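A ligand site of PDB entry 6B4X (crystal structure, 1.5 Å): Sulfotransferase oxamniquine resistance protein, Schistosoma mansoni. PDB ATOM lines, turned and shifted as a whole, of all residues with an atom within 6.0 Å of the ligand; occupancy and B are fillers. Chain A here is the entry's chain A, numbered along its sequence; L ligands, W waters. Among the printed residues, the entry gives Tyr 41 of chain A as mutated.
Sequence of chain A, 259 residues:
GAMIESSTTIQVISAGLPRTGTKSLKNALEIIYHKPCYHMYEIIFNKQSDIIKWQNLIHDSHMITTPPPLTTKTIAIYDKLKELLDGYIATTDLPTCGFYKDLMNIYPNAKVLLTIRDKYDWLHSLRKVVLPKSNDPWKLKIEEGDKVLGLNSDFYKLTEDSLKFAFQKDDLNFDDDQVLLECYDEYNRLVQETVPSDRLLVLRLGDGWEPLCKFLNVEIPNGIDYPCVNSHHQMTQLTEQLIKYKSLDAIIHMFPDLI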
ATOM      1  N   LEU A  17     -32.706 -32.328 -25.654  1.00  0.00           N
ATOM      2  CA  LEU A  17     -32.115 -33.006 -26.810  1.00  0.00           C
ATOM      3  C   LEU A  17     -30.607 -32.716 -26.937  1.00  0.00           C
ATOM      4  O   LEU A  17     -30.094 -31.743 -26.398  1.00  0.00           O
ATOM      5  CB  LEU A  17     -32.851 -32.581 -28.088  1.00  0.00           C
ATOM      6  CG  LEU A  17     -34.286 -33.106 -28.240  1.00  0.00           C
ATOM      7  CD1 LEU A  17     -35.065 -32.371 -29.347  1.00  0.00           C
ATOM      8  CD2 LEU A  17     -34.342 -34.640 -28.445  1.00  0.00           C
ATOM      9  N   PRO A  18     -29.891 -33.562 -27.686  1.00  0.00           N
ATOM     10  CA  PRO A  18     -28.486 -33.204 -27.944  1.00  0.00           C
ATOM     11  C   PRO A  18     -28.329 -31.804 -28.551  1.00  0.00           C
ATOM     12  O   PRO A  18     -29.195 -31.358 -29.293  1.00  0.00           O
ATOM     13  CB  PRO A  18     -28.034 -34.269 -28.967  1.00  0.00           C
ATOM     14  CG  PRO A  18     -29.287 -34.971 -29.415  1.00  0.00           C
ATOM     15  CD  PRO A  18     -30.279 -34.840 -28.310  1.00  0.00           C
ATOM     16  N   ARG A  19     -27.226 -31.142 -28.205  1.00  0.00           N
ATOM     17  CA  ARG A  19     -26.895 -29.797 -28.666  1.00  0.00           C
ATOM     18  C   ARG A  19     -27.765 -28.719 -28.016  1.00  0.00           C
ATOM     19  O   ARG A  19     -27.976 -27.640 -28.591  1.00  0.00           O
ATOM     20  CB  ARG A  19     -26.902 -29.677 -30.192  1.00  0.00           C
ATOM     21  CG  ARG A  19     -26.089 -30.762 -30.905  1.00  0.00           C
ATOM     22  CD  ARG A  19     -24.684 -30.964 -30.312  1.00  0.00           C
ATOM     23  NE  ARG A  19     -23.820 -29.792 -30.514  1.00  0.00           N
ATOM     24  CZ  ARG A  19     -22.627 -29.642 -29.952  1.00  0.00           C
ATOM     25  NH1 ARG A  19     -22.134 -30.586 -29.139  1.00  0.00           N
ATOM     26  NH2 ARG A  19     -21.905 -28.555 -30.203  1.00  0.00           N
ATOM     27  N   THR A  20     -28.245 -28.998 -26.809  1.00  0.00           N
ATOM     28  CA  THR A  20     -28.985 -27.995 -26.038  1.00  0.00           C
ATOM     29  C   THR A  20     -28.332 -27.666 -24.703  1.00  0.00           C
ATOM     30  O   THR A  20     -28.984 -27.158 -23.780  1.00  0.00           O
ATOM     31  CB  THR A  20     -30.471 -28.419 -25.773  1.00  0.00           C
ATOM     32  OG1 THR A  20     -30.504 -29.600 -24.972  1.00  0.00           O
ATOM     33  CG2 THR A  20     -31.225 -28.645 -27.109  1.00  0.00           C
ATOM     34  N   GLY A  21     -27.033 -27.911 -24.595  1.00  0.00           N
ATOM     35  CA  GLY A  21     -26.299 -27.666 -23.355  1.00  0.00           C
ATOM     36  C   GLY A  21     -26.245 -28.857 -22.413  1.00  0.00           C
ATOM     37  O   GLY A  21     -26.076 -28.678 -21.202  1.00  0.00           O
ATOM     38  N   THR A  22     -26.365 -30.066 -22.951  1.00  0.00           N
ATOM     39  CA  THR A  22     -26.401 -31.271 -22.121  1.00  0.00           C
ATOM     40  C   THR A  22     -25.058 -31.546 -21.445  1.00  0.00           C
ATOM     41  O   THR A  22     -25.031 -32.024 -20.310  1.00  0.00           O
ATOM     42  CB  THR A  22     -26.850 -32.524 -22.917  1.00  0.00           C
ATOM     43  OG1 THR A  22     -25.869 -32.858 -23.923  1.00  0.00           O
ATOM     44  CG2 THR A  22     -28.219 -32.322 -23.583  1.00  0.00           C
ATOM     45  N   LYS A  23     -23.957 -31.283 -22.124  1.00  0.00           N
ATOM     46  CA  LYS A  23     -22.645 -31.563 -21.521  1.00  0.00           C
ATOM     47  C   LYS A  23     -22.348 -30.568 -20.410  1.00  0.00           C
ATOM     48  O   LYS A  23     -21.826 -30.952 -19.355  1.00  0.00           O
ATOM     49  CB  LYS A  23     -21.532 -31.621 -22.578  1.00  0.00           C
ATOM     50  CG  LYS A  23     -20.169 -31.989 -22.052  1.00  0.00           C
ATOM     51  CD  LYS A  23     -20.200 -33.273 -21.231  1.00  0.00           C
ATOM     52  CE  LYS A  23     -18.820 -33.894 -21.048  1.00  0.00           C
ATOM     53  NZ  LYS A  23     -17.920 -33.206 -20.067  1.00  0.00           N
ATOM     54  N   SER A  24     -22.683 -29.296 -20.625  1.00  0.00           N
ATOM     55  CA  SER A  24     -22.543 -28.306 -19.558  1.00  0.00           C
ATOM     56  C   SER A  24     -23.401 -28.692 -18.350  1.00  0.00           C
ATOM     57  O   SER A  24     -22.964 -28.547 -17.205  1.00  0.00           O
ATOM     58  CB  SER A  24     -22.953 -26.920 -20.030  1.00  0.00           C
ATOM     59  OG  SER A  24     -21.987 -26.409 -20.942  1.00  0.00           O
ATOM     60  N   HIS A  39     -24.416 -39.359 -19.817  1.00  0.00           N
ATOM     61  CA  HIS A  39     -24.370 -38.498 -20.995  1.00  0.00           C
ATOM     62  C   HIS A  39     -23.822 -39.396 -22.104  1.00  0.00           C
ATOM     63  O   HIS A  39     -23.230 -40.427 -21.806  1.00  0.00           O
ATOM     64  CB  HIS A  39     -23.414 -37.343 -20.728  1.00  0.00           C
ATOM     65  CG  HIS A  39     -23.385 -36.302 -21.810  1.00  0.00           C
ATOM     66  ND1 HIS A  39     -22.548 -36.383 -22.916  1.00  0.00           N
ATOM     67  CD2 HIS A  39     -24.079 -35.154 -21.950  1.00  0.00           C
ATOM     68  CE1 HIS A  39     -22.753 -35.333 -23.684  1.00  0.00           C
ATOM     69  NE2 HIS A  39     -23.674 -34.561 -23.126  1.00  0.00           N
ATOM     70  N   TYR A  41     -21.230 -38.889 -23.689  1.00  0.00           N
ATOM     71  CA  TYR A  41     -19.788 -38.923 -23.491  1.00  0.00           C
ATOM     72  C   TYR A  41     -19.379 -39.942 -22.416  1.00  0.00           C
ATOM     73  O   TYR A  41     -18.270 -40.487 -22.456  1.00  0.00           O
ATOM     74  CB  TYR A  41     -19.243 -37.517 -23.188  1.00  0.00           C
ATOM     75  CG  TYR A  41     -19.299 -36.552 -24.367  1.00  0.00           C
ATOM     76  CD1 TYR A  41     -19.975 -36.871 -25.543  1.00  0.00           C
ATOM     77  CD2 TYR A  41     -18.653 -35.324 -24.309  1.00  0.00           C
ATOM     78  CE1 TYR A  41     -20.038 -35.989 -26.614  1.00  0.00           C
ATOM     79  CE2 TYR A  41     -18.703 -34.443 -25.363  1.00  0.00           C
ATOM     80  CZ  TYR A  41     -19.392 -34.766 -26.512  1.00  0.00           C
ATOM     81  OH  TYR A  41     -19.430 -33.854 -27.567  1.00  0.00           O
ATOM     82  N   ASP A  93     -28.814 -36.117 -22.293  1.00  0.00           N
ATOM     83  CA  ASP A  93     -28.396 -36.451 -23.653  1.00  0.00           C
ATOM     84  C   ASP A  93     -29.020 -37.746 -24.182  1.00  0.00           C
ATOM     85  O   ASP A  93     -29.718 -38.461 -23.449  1.00  0.00           O
ATOM     86  CB  ASP A  93     -26.850 -36.502 -23.687  1.00  0.00           C
ATOM     87  CG  ASP A  93     -26.254 -36.417 -25.079  1.00  0.00           C
ATOM     88  OD1 ASP A  93     -26.982 -36.164 -26.074  1.00  0.00           O
ATOM     89  OD2 ASP A  93     -25.030 -36.616 -25.158  1.00  0.00           O
ATOM     90  N   ARG A 117     -33.305 -24.280 -26.833  1.00  0.00           N
ATOM     91  CA  ARG A 117     -32.650 -23.145 -27.470  1.00  0.00           C
ATOM     92  C   ARG A 117     -33.323 -22.851 -28.803  1.00  0.00           C
ATOM     93  O   ARG A 117     -34.196 -23.607 -29.251  1.00  0.00           O
ATOM     94  CB  ARG A 117     -31.163 -23.452 -27.694  1.00  0.00           C
ATOM     95  CG  ARG A 117     -30.930 -24.473 -28.795  1.00  0.00           C
ATOM     96  CD  ARG A 117     -29.479 -24.906 -28.898  1.00  0.00           C
ATOM     97  NE  ARG A 117     -28.568 -23.822 -29.282  1.00  0.00           N
ATOM     98  CZ  ARG A 117     -27.300 -24.021 -29.609  1.00  0.00           C
ATOM     99  NH1 ARG A 117     -26.798 -25.256 -29.621  1.00  0.00           N
ATOM    100  NH2 ARG A 117     -26.520 -22.993 -29.931  1.00  0.00           N
ATOM    101  N   ASP A 121     -30.341 -22.476 -34.384  1.00  0.00           N
ATOM    102  CA  ASP A 121     -29.031 -22.661 -33.734  1.00  0.00           C
ATOM    103  C   ASP A 121     -28.843 -24.138 -33.396  1.00  0.00           C
ATOM    104  O   ASP A 121     -27.761 -24.690 -33.562  1.00  0.00           O
ATOM    105  CB  ASP A 121     -28.932 -21.850 -32.443  1.00  0.00           C
ATOM    106  CG  ASP A 121     -28.853 -20.337 -32.668  1.00  0.00           C
ATOM    107  OD1 ASP A 121     -28.555 -19.887 -33.804  1.00  0.00           O
ATOM    108  OD2 ASP A 121     -29.063 -19.595 -31.674  1.00  0.00           O
ATOM    109  N   HIS A 124     -28.137 -26.093 -36.671  1.00  0.00           N
ATOM    110  CA  HIS A 124     -26.783 -25.789 -37.119  1.00  0.00           C
ATOM    111  C   HIS A 124     -25.747 -26.555 -36.305  1.00  0.00           C
ATOM    112  O   HIS A 124     -24.824 -27.154 -36.871  1.00  0.00           O
ATOM    113  CB  HIS A 124     -26.577 -24.289 -36.968  1.00  0.00           C
ATOM    114  CG  HIS A 124     -25.236 -23.803 -37.418  1.00  0.00           C
ATOM    115  ND1 HIS A 124     -24.251 -23.421 -36.530  1.00  0.00           N
ATOM    116  CD2 HIS A 124     -24.742 -23.591 -38.650  1.00  0.00           C
ATOM    117  CE1 HIS A 124     -23.188 -23.010 -37.206  1.00  0.00           C
ATOM    118  NE2 HIS A 124     -23.453 -23.106 -38.497  1.00  0.00           N
ATOM    119  N   SER A 125     -25.909 -26.562 -34.981  1.00  0.00           N
ATOM    120  CA  SER A 125     -25.020 -27.268 -34.074  1.00  0.00           C
ATOM    121  C   SER A 125     -25.073 -28.779 -34.309  1.00  0.00           C
ATOM    122  O   SER A 125     -24.049 -29.457 -34.376  1.00  0.00           O
ATOM    123  CB  SER A 125     -25.433 -26.943 -32.634  1.00  0.00           C
ATOM    124  OG  SER A 125     -24.492 -27.426 -31.703  1.00  0.00           O
ATOM    125  N   VAL A 129     -21.927 -31.601 -35.545  1.00  0.00           N
ATOM    126  CA  VAL A 129     -21.382 -32.513 -34.544  1.00  0.00           C
ATOM    127  C   VAL A 129     -22.012 -33.908 -34.540  1.00  0.00           C
ATOM    128  O   VAL A 129     -21.306 -34.908 -34.541  1.00  0.00           O
ATOM    129  CB  VAL A 129     -21.537 -31.896 -33.115  1.00  0.00           C
ATOM    130  CG1 VAL A 129     -20.982 -32.835 -32.046  1.00  0.00           C
ATOM    131  CG2 VAL A 129     -20.833 -30.545 -33.044  1.00  0.00           C
ATOM    132  N   VAL A 130     -23.338 -33.972 -34.516  1.00  0.00           N
ATOM    133  CA  VAL A 130     -24.054 -35.220 -34.251  1.00  0.00           C
ATOM    134  C   VAL A 130     -24.575 -35.840 -35.530  1.00  0.00           C
ATOM    135  O   VAL A 130     -24.513 -37.066 -35.711  1.00  0.00           O
ATOM    136  CB  VAL A 130     -25.259 -34.945 -33.309  1.00  0.00           C
ATOM    137  CG1 VAL A 130     -26.098 -36.225 -33.109  1.00  0.00           C
ATOM    138  CG2 VAL A 130     -24.752 -34.443 -31.975  1.00  0.00           C
ATOM    139  N   LEU A 205     -30.294 -21.850 -22.719  1.00  0.00           N
ATOM    140  CA  LEU A 205     -28.841 -21.663 -22.686  1.00  0.00           C
ATOM    141  C   LEU A 205     -28.550 -20.282 -22.139  1.00  0.00           C
ATOM    142  O   LEU A 205     -29.187 -19.312 -22.547  1.00  0.00           O
ATOM    143  CB  LEU A 205     -28.218 -21.777 -24.082  1.00  0.00           C
ATOM    144  CG  LEU A 205     -28.091 -23.173 -24.683  1.00  0.00           C
ATOM    145  CD1 LEU A 205     -27.505 -23.075 -26.100  1.00  0.00           C
ATOM    146  CD2 LEU A 205     -27.264 -24.094 -23.782  1.00  0.00           C
ATOM    147  N   GLY A 206     -27.635 -20.183 -21.193  1.00  0.00           N
ATOM    148  CA  GLY A 206     -27.309 -18.916 -20.601  1.00  0.00           C
ATOM    149  C   GLY A 206     -27.950 -18.668 -19.239  1.00  0.00           C
ATOM    150  O   GLY A 206     -27.565 -17.730 -18.554  1.00  0.00           O
ATOM    151  N   TYR A 226     -20.877 -21.342 -14.063  1.00  0.00           N
ATOM    152  CA  TYR A 226     -21.669 -22.360 -14.735  1.00  0.00           C
ATOM    153  C   TYR A 226     -20.929 -22.803 -15.998  1.00  0.00           C
ATOM    154  O   TYR A 226     -20.410 -21.969 -16.734  1.00  0.00           O
ATOM    155  CB  TYR A 226     -23.073 -21.844 -15.069  1.00  0.00           C
ATOM    156  CG  TYR A 226     -23.957 -22.946 -15.596  1.00  0.00           C
ATOM    157  CD1 TYR A 226     -24.712 -23.741 -14.723  1.00  0.00           C
ATOM    158  CD2 TYR A 226     -24.017 -23.221 -16.958  1.00  0.00           C
ATOM    159  CE1 TYR A 226     -25.489 -24.760 -15.198  1.00  0.00           C
ATOM    160  CE2 TYR A 226     -24.781 -24.249 -17.438  1.00  0.00           C
ATOM    161  CZ  TYR A 226     -25.530 -25.004 -16.556  1.00  0.00           C
ATOM    162  OH  TYR A 226     -26.311 -26.032 -17.045  1.00  0.00           O
ATOM    163  N   PRO A 227     -20.842 -24.133 -16.228  1.00  0.00           N
ATOM    164  CA  PRO A 227     -20.053 -24.628 -17.361  1.00  0.00           C
ATOM    165  C   PRO A 227     -20.525 -24.125 -18.723  1.00  0.00           C
ATOM    166  O   PRO A 227     -21.720 -23.970 -18.950  1.00  0.00           O
ATOM    167  CB  PRO A 227     -20.243 -26.154 -17.272  1.00  0.00           C
ATOM    168  CG  PRO A 227     -20.536 -26.398 -15.812  1.00  0.00           C
ATOM    169  CD  PRO A 227     -21.370 -25.220 -15.398  1.00  0.00           C
ATOM    170  N   CAS A 228     -19.556 -23.841 -19.587  1.00  0.00           N
ATOM    171  CA  CAS A 228     -19.848 -23.555 -20.970  1.00  0.00           C
ATOM    172  CB  CAS A 228     -19.622 -22.100 -21.310  1.00  0.00           C
ATOM    173  C   CAS A 228     -18.882 -24.402 -21.731  1.00  0.00           C
ATOM    174  O   CAS A 228     -17.717 -24.010 -21.910  1.00  0.00           O
ATOM    175  SG  CAS A 228     -20.206 -21.885 -22.959  1.00  0.00           S
ATOM    176 AS   CAS A 228     -18.285 -21.633 -24.035  1.00  0.00          AS
ATOM    177  CE1 CAS A 228     -17.996 -23.067 -25.371  1.00  0.00           C
ATOM    178  CE2 CAS A 228     -18.506 -19.890 -24.968  1.00  0.00           C
ATOM    179  N   VAL A 229     -19.330 -25.577 -22.145  1.00  0.00           N
ATOM    180  CA  VAL A 229     -18.465 -26.517 -22.856  1.00  0.00           C
ATOM    181  C   VAL A 229     -19.186 -27.153 -24.022  1.00  0.00           C
ATOM    182  O   VAL A 229     -20.421 -27.053 -24.143  1.00  0.00           O
ATOM    183  CB  VAL A 229     -17.988 -27.669 -21.913  1.00  0.00           C
ATOM    184  CG1 VAL A 229     -17.117 -27.138 -20.801  1.00  0.00           C
ATOM    185  CG2 VAL A 229     -19.190 -28.429 -21.356  1.00  0.00           C
ATOM    186  N   ASN A 230     -18.421 -27.809 -24.899  1.00  0.00           N
ATOM    187  CA  ASN A 230     -18.966 -28.645 -25.963  1.00  0.00           C
ATOM    188  C   ASN A 230     -19.535 -27.847 -27.138  1.00  0.00           C
ATOM    189  O   ASN A 230     -20.450 -28.310 -27.801  1.00  0.00           O
ATOM    190  CB  ASN A 230     -19.989 -29.646 -25.398  1.00  0.00           C
ATOM    191  CG  ASN A 230     -20.068 -30.934 -26.197  1.00  0.00           C
ATOM    192  OD1 ASN A 230     -19.095 -31.342 -26.823  1.00  0.00           O
ATOM    193  ND2 ASN A 230     -21.219 -31.593 -26.151  1.00  0.00           N
ATOM    194  N   SER A 231     -18.999 -26.654 -27.375  1.00  0.00           N
ATOM    195  CA  SER A 231     -19.419 -25.878 -28.536  1.00  0.00           C
ATOM    196  C   SER A 231     -19.034 -26.616 -29.814  1.00  0.00           C
ATOM    197  O   SER A 231     -18.122 -27.431 -29.810  1.00  0.00           O
ATOM    198  CB  SER A 231     -18.756 -24.498 -28.560  1.00  0.00           C
ATOM    199  OG  SER A 231     -17.362 -24.579 -28.785  1.00  0.00           O
ATOM    200  N   HIS A 232     -19.715 -26.339 -30.906  1.00  0.00           N
ATOM    201  CA  HIS A 232     -19.327 -27.001 -32.148  1.00  0.00           C
ATOM    202  C   HIS A 232     -17.906 -26.626 -32.553  1.00  0.00           C
ATOM    203  O   HIS A 232     -17.209 -27.452 -33.129  1.00  0.00           O
ATOM    204  CB  HIS A 232     -20.346 -26.822 -33.297  1.00  0.00           C
ATOM    205  CG  HIS A 232     -20.431 -25.425 -33.843  1.00  0.00           C
ATOM    206  ND1 HIS A 232     -19.487 -24.900 -34.708  1.00  0.00           N
ATOM    207  CD2 HIS A 232     -21.345 -24.451 -33.645  1.00  0.00           C
ATOM    208  CE1 HIS A 232     -19.829 -23.668 -35.022  1.00  0.00           C
ATOM    209  NE2 HIS A 232     -20.950 -23.371 -34.407  1.00  0.00           N
ATOM    210  N   HIS A 233     -17.466 -25.388 -32.258  1.00  0.00           N
ATOM    211  CA  HIS A 233     -16.099 -25.016 -32.577  1.00  0.00           C
ATOM    212  C   HIS A 233     -15.099 -25.897 -31.843  1.00  0.00           C
ATOM    213  O   HIS A 233     -14.098 -26.329 -32.414  1.00  0.00           O
ATOM    214  CB  HIS A 233     -15.832 -23.544 -32.232  1.00  0.00           C
ATOM    215  CG  HIS A 233     -16.610 -22.567 -33.056  1.00  0.00           C
ATOM    216  ND1 HIS A 233     -16.450 -22.454 -34.422  1.00  0.00           N
ATOM    217  CD2 HIS A 233     -17.512 -21.630 -32.700  1.00  0.00           C
ATOM    218  CE1 HIS A 233     -17.249 -21.491 -34.865  1.00  0.00           C
ATOM    219  NE2 HIS A 233     -17.904 -20.985 -33.844  1.00  0.00           N
HETATM  220  P1  LIG L   1     -23.045 -24.580 -30.286  1.00  0.00           P
HETATM  221  O1  LIG L   1     -24.030 -23.784 -31.069  1.00  0.00           O
HETATM  222  O2  LIG L   1     -22.649 -25.852 -31.029  1.00  0.00           O
HETATM  223  O3  LIG L   1     -21.787 -23.824 -29.872  1.00  0.00           O
HETATM  224  P2  LIG L   1     -24.593 -30.323 -25.971  1.00  0.00           P
HETATM  225  O4  LIG L   1     -25.961 -30.816 -25.558  1.00  0.00           O
HETATM  226  O5  LIG L   1     -23.613 -30.382 -24.836  1.00  0.00           O
HETATM  227  O6  LIG L   1     -24.072 -31.089 -27.187  1.00  0.00           O
HETATM  228  O7  LIG L   1     -24.773 -28.762 -26.327  1.00  0.00           O
HETATM  229  C1  LIG L   1     -23.680 -27.981 -26.778  1.00  0.00           C
HETATM  230  C2  LIG L   1     -24.213 -26.646 -27.227  1.00  0.00           C
HETATM  231  O8  LIG L   1     -24.629 -25.846 -26.068  1.00  0.00           O
HETATM  232  C3  LIG L   1     -23.168 -25.831 -27.921  1.00  0.00           C
HETATM  233  O9  LIG L   1     -23.813 -25.035 -28.942  1.00  0.00           O
HETATM  234  C4  LIG L   1     -22.640 -25.000 -26.822  1.00  0.00           C
HETATM  235  O10 LIG L   1     -21.914 -23.844 -27.241  1.00  0.00           O
HETATM  236  C5  LIG L   1     -23.869 -24.635 -26.058  1.00  0.00           C
HETATM  237  N1  LIG L   1     -23.642 -24.318 -24.698  1.00  0.00           N
HETATM  238  C6  LIG L   1     -23.222 -25.163 -23.738  1.00  0.00           C
HETATM  239  N2  LIG L   1     -23.126 -24.500 -22.572  1.00  0.00           N
HETATM  240  C7  LIG L   1     -23.498 -23.211 -22.781  1.00  0.00           C
HETATM  241  C8  LIG L   1     -23.599 -22.050 -21.953  1.00  0.00           C
HETATM  242  N3  LIG L   1     -23.285 -22.132 -20.575  1.00  0.00           N
HETATM  243  N4  LIG L   1     -24.042 -20.918 -22.512  1.00  0.00           N
HETATM  244  C9  LIG L   1     -24.341 -20.845 -23.806  1.00  0.00           C
HETATM  245  N5  LIG L   1     -24.258 -21.877 -24.623  1.00  0.00           N
HETATM  246  C10 LIG L   1     -23.851 -23.082 -24.149  1.00  0.00           C
HETATM  247  O   HOH W   1     -25.974 -21.165 -18.609  1.00  0.00           O
HETATM  248  O   HOH W   2     -25.144 -33.743 -27.560  1.00  0.00           O
HETATM  249  O   HOH W   3     -23.921 -18.280 -21.586  1.00  0.00           O
HETATM  250  O   HOH W   4     -20.481 -21.665 -26.545  1.00  0.00           O
HETATM  251  O   HOH W   5     -24.514 -20.594 -27.146  1.00  0.00           O
HETATM  252  O   HOH W   6     -25.272 -23.273 -33.426  1.00  0.00           O
HETATM  253  O   HOH W   7     -23.688 -21.154 -29.755  1.00  0.00           O
HETATM  254  O   HOH W   8     -20.189 -22.213 -30.942  1.00  0.00           O
HETATM  255  O   HOH W   9     -22.919 -28.313 -23.339  1.00  0.00           O
HETATM  256  O   HOH W  10     -23.693 -19.857 -18.523  1.00  0.00           O
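The guanidinium group (NE) of Arg 19 sits at hydrogen-bond distance from the side-chain hydroxyl (OG) of Ser 125 (2.7 Å). The side-chain hydroxyl (OG1) of Thr 22 is in hydrogen-bond range of a ring nitrogen (NE2) of His 39, at 2.9 Å. The side-chain hydroxyl (OG) of Ser 24 sits at hydrogen-bond distance from the backbone NH (N) of Val 229, at 3.0 Å. The backbone carbonyl oxygen (O) of Arg 19 sits at hydrogen-bond distance from the guanidinium group (NH1) of Arg 117, 2.9 Å away. NH2 of Arg 19 sits at hydrogen-bond distance from O of Asn 230. The backbone NH (N) of Lys 23 lies within hydrogen-bond range of a ring nitrogen (NE2) of His 39. The side-chain amide oxygen (OD1) of Asn 230 sits at hydrogen-bond distance from the side-chain hydroxyl (OH) of Tyr 41 (2.6 Å). O of Leu 17 is in hydrogen-bond range of OG1 of Thr 20, at 2.6 Å.
Water W9 lies within hydrogen-bond range of O5 of the ligand, N of Ser 24, O of Val 229 and N of Lys 23. Water W4 lies within hydrogen-bond range of an oxygen (O10) of the ligand (2.7 Å) and SG of CAS 228 (3.6 Å). Water W6 lies within hydrogen-bond range of an oxygen (O1) of the ligand, the backbone carbonyl oxygen (O) of Asp 121 and a ring nitrogen (ND1) of His 124. Water W2 lies within hydrogen-bond range of an oxygen (O6) of the ligand (2.9 Å), the side-chain carboxylate (OD1) of Asp 93 (3.4 Å) and the backbone NH (N) of Arg 19 (3.4 Å). Water W7 bridges O1 of the ligand (3.0 Å) and NH2 of Arg 117 (3.4 Å). Water W1 lies within hydrogen-bond range of N of Gly 206 (3.2 Å) and N3 of the ligand (3.5 Å).
O2 of the ligand is in hydrogen-bond range of OG of Ser 125 (2.5 Å). The backbone NH of Thr 22 is in hydrogen-bond range of an oxygen (O4) of the ligand, 2.7 Å away. An oxygen (O4) of the ligand sits at hydrogen-bond distance from the side-chain hydroxyl of Thr 22. OG of Ser 24 sits at hydrogen-bond distance from N2 of the ligand (2.8 Å). O4 of the ligand is in hydrogen-bond range of N of Arg 19, 3.0 Å away. The guanidinium group (NH1) of Arg 19 is in salt-bridge range of an oxygen (O6) of the ligand (2.8 Å). An oxygen (O1) of the ligand lies within salt-bridge range of the guanidinium group of Arg 117, at 2.8 Å. The backbone NH (N) of Lys 23 lies within hydrogen-bond range of an oxygen (O5) of the ligand, at 2.9 Å. O of Pro 227 sits at hydrogen-bond distance from N3 of the ligand. N of Gly 21 lies within hydrogen-bond range of O7 of the ligand (3.0 Å). An oxygen (O2) of the ligand lies within hydrogen-bond range of the backbone NH (N) of His 232. O5 of the ligand lies within hydrogen-bond range of ND2 of Asn 230, 3.0 Å away. An oxygen (O4) of the ligand lies within hydrogen-bond range of the backbone NH (N) of Thr 20, at 3.2 Å.
C of Pro 18 touches O4 of the ligand, at 3.9 Å. CD2 of Leu 205 touches C10 of the ligand, at 3.6 Å. N of Gly 206 touches N4 of the ligand (3.9 Å). Tyr 226 touches the ligand (CD2 to N3, 3.8 Å). CAS 228 touches the ligand. Val 229 touches the ligand. CB of Ser 231 touches O3 of the ligand, at 3.4 Å. Of the 27 residues printed, 18 come within 4 Å of the ligand.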
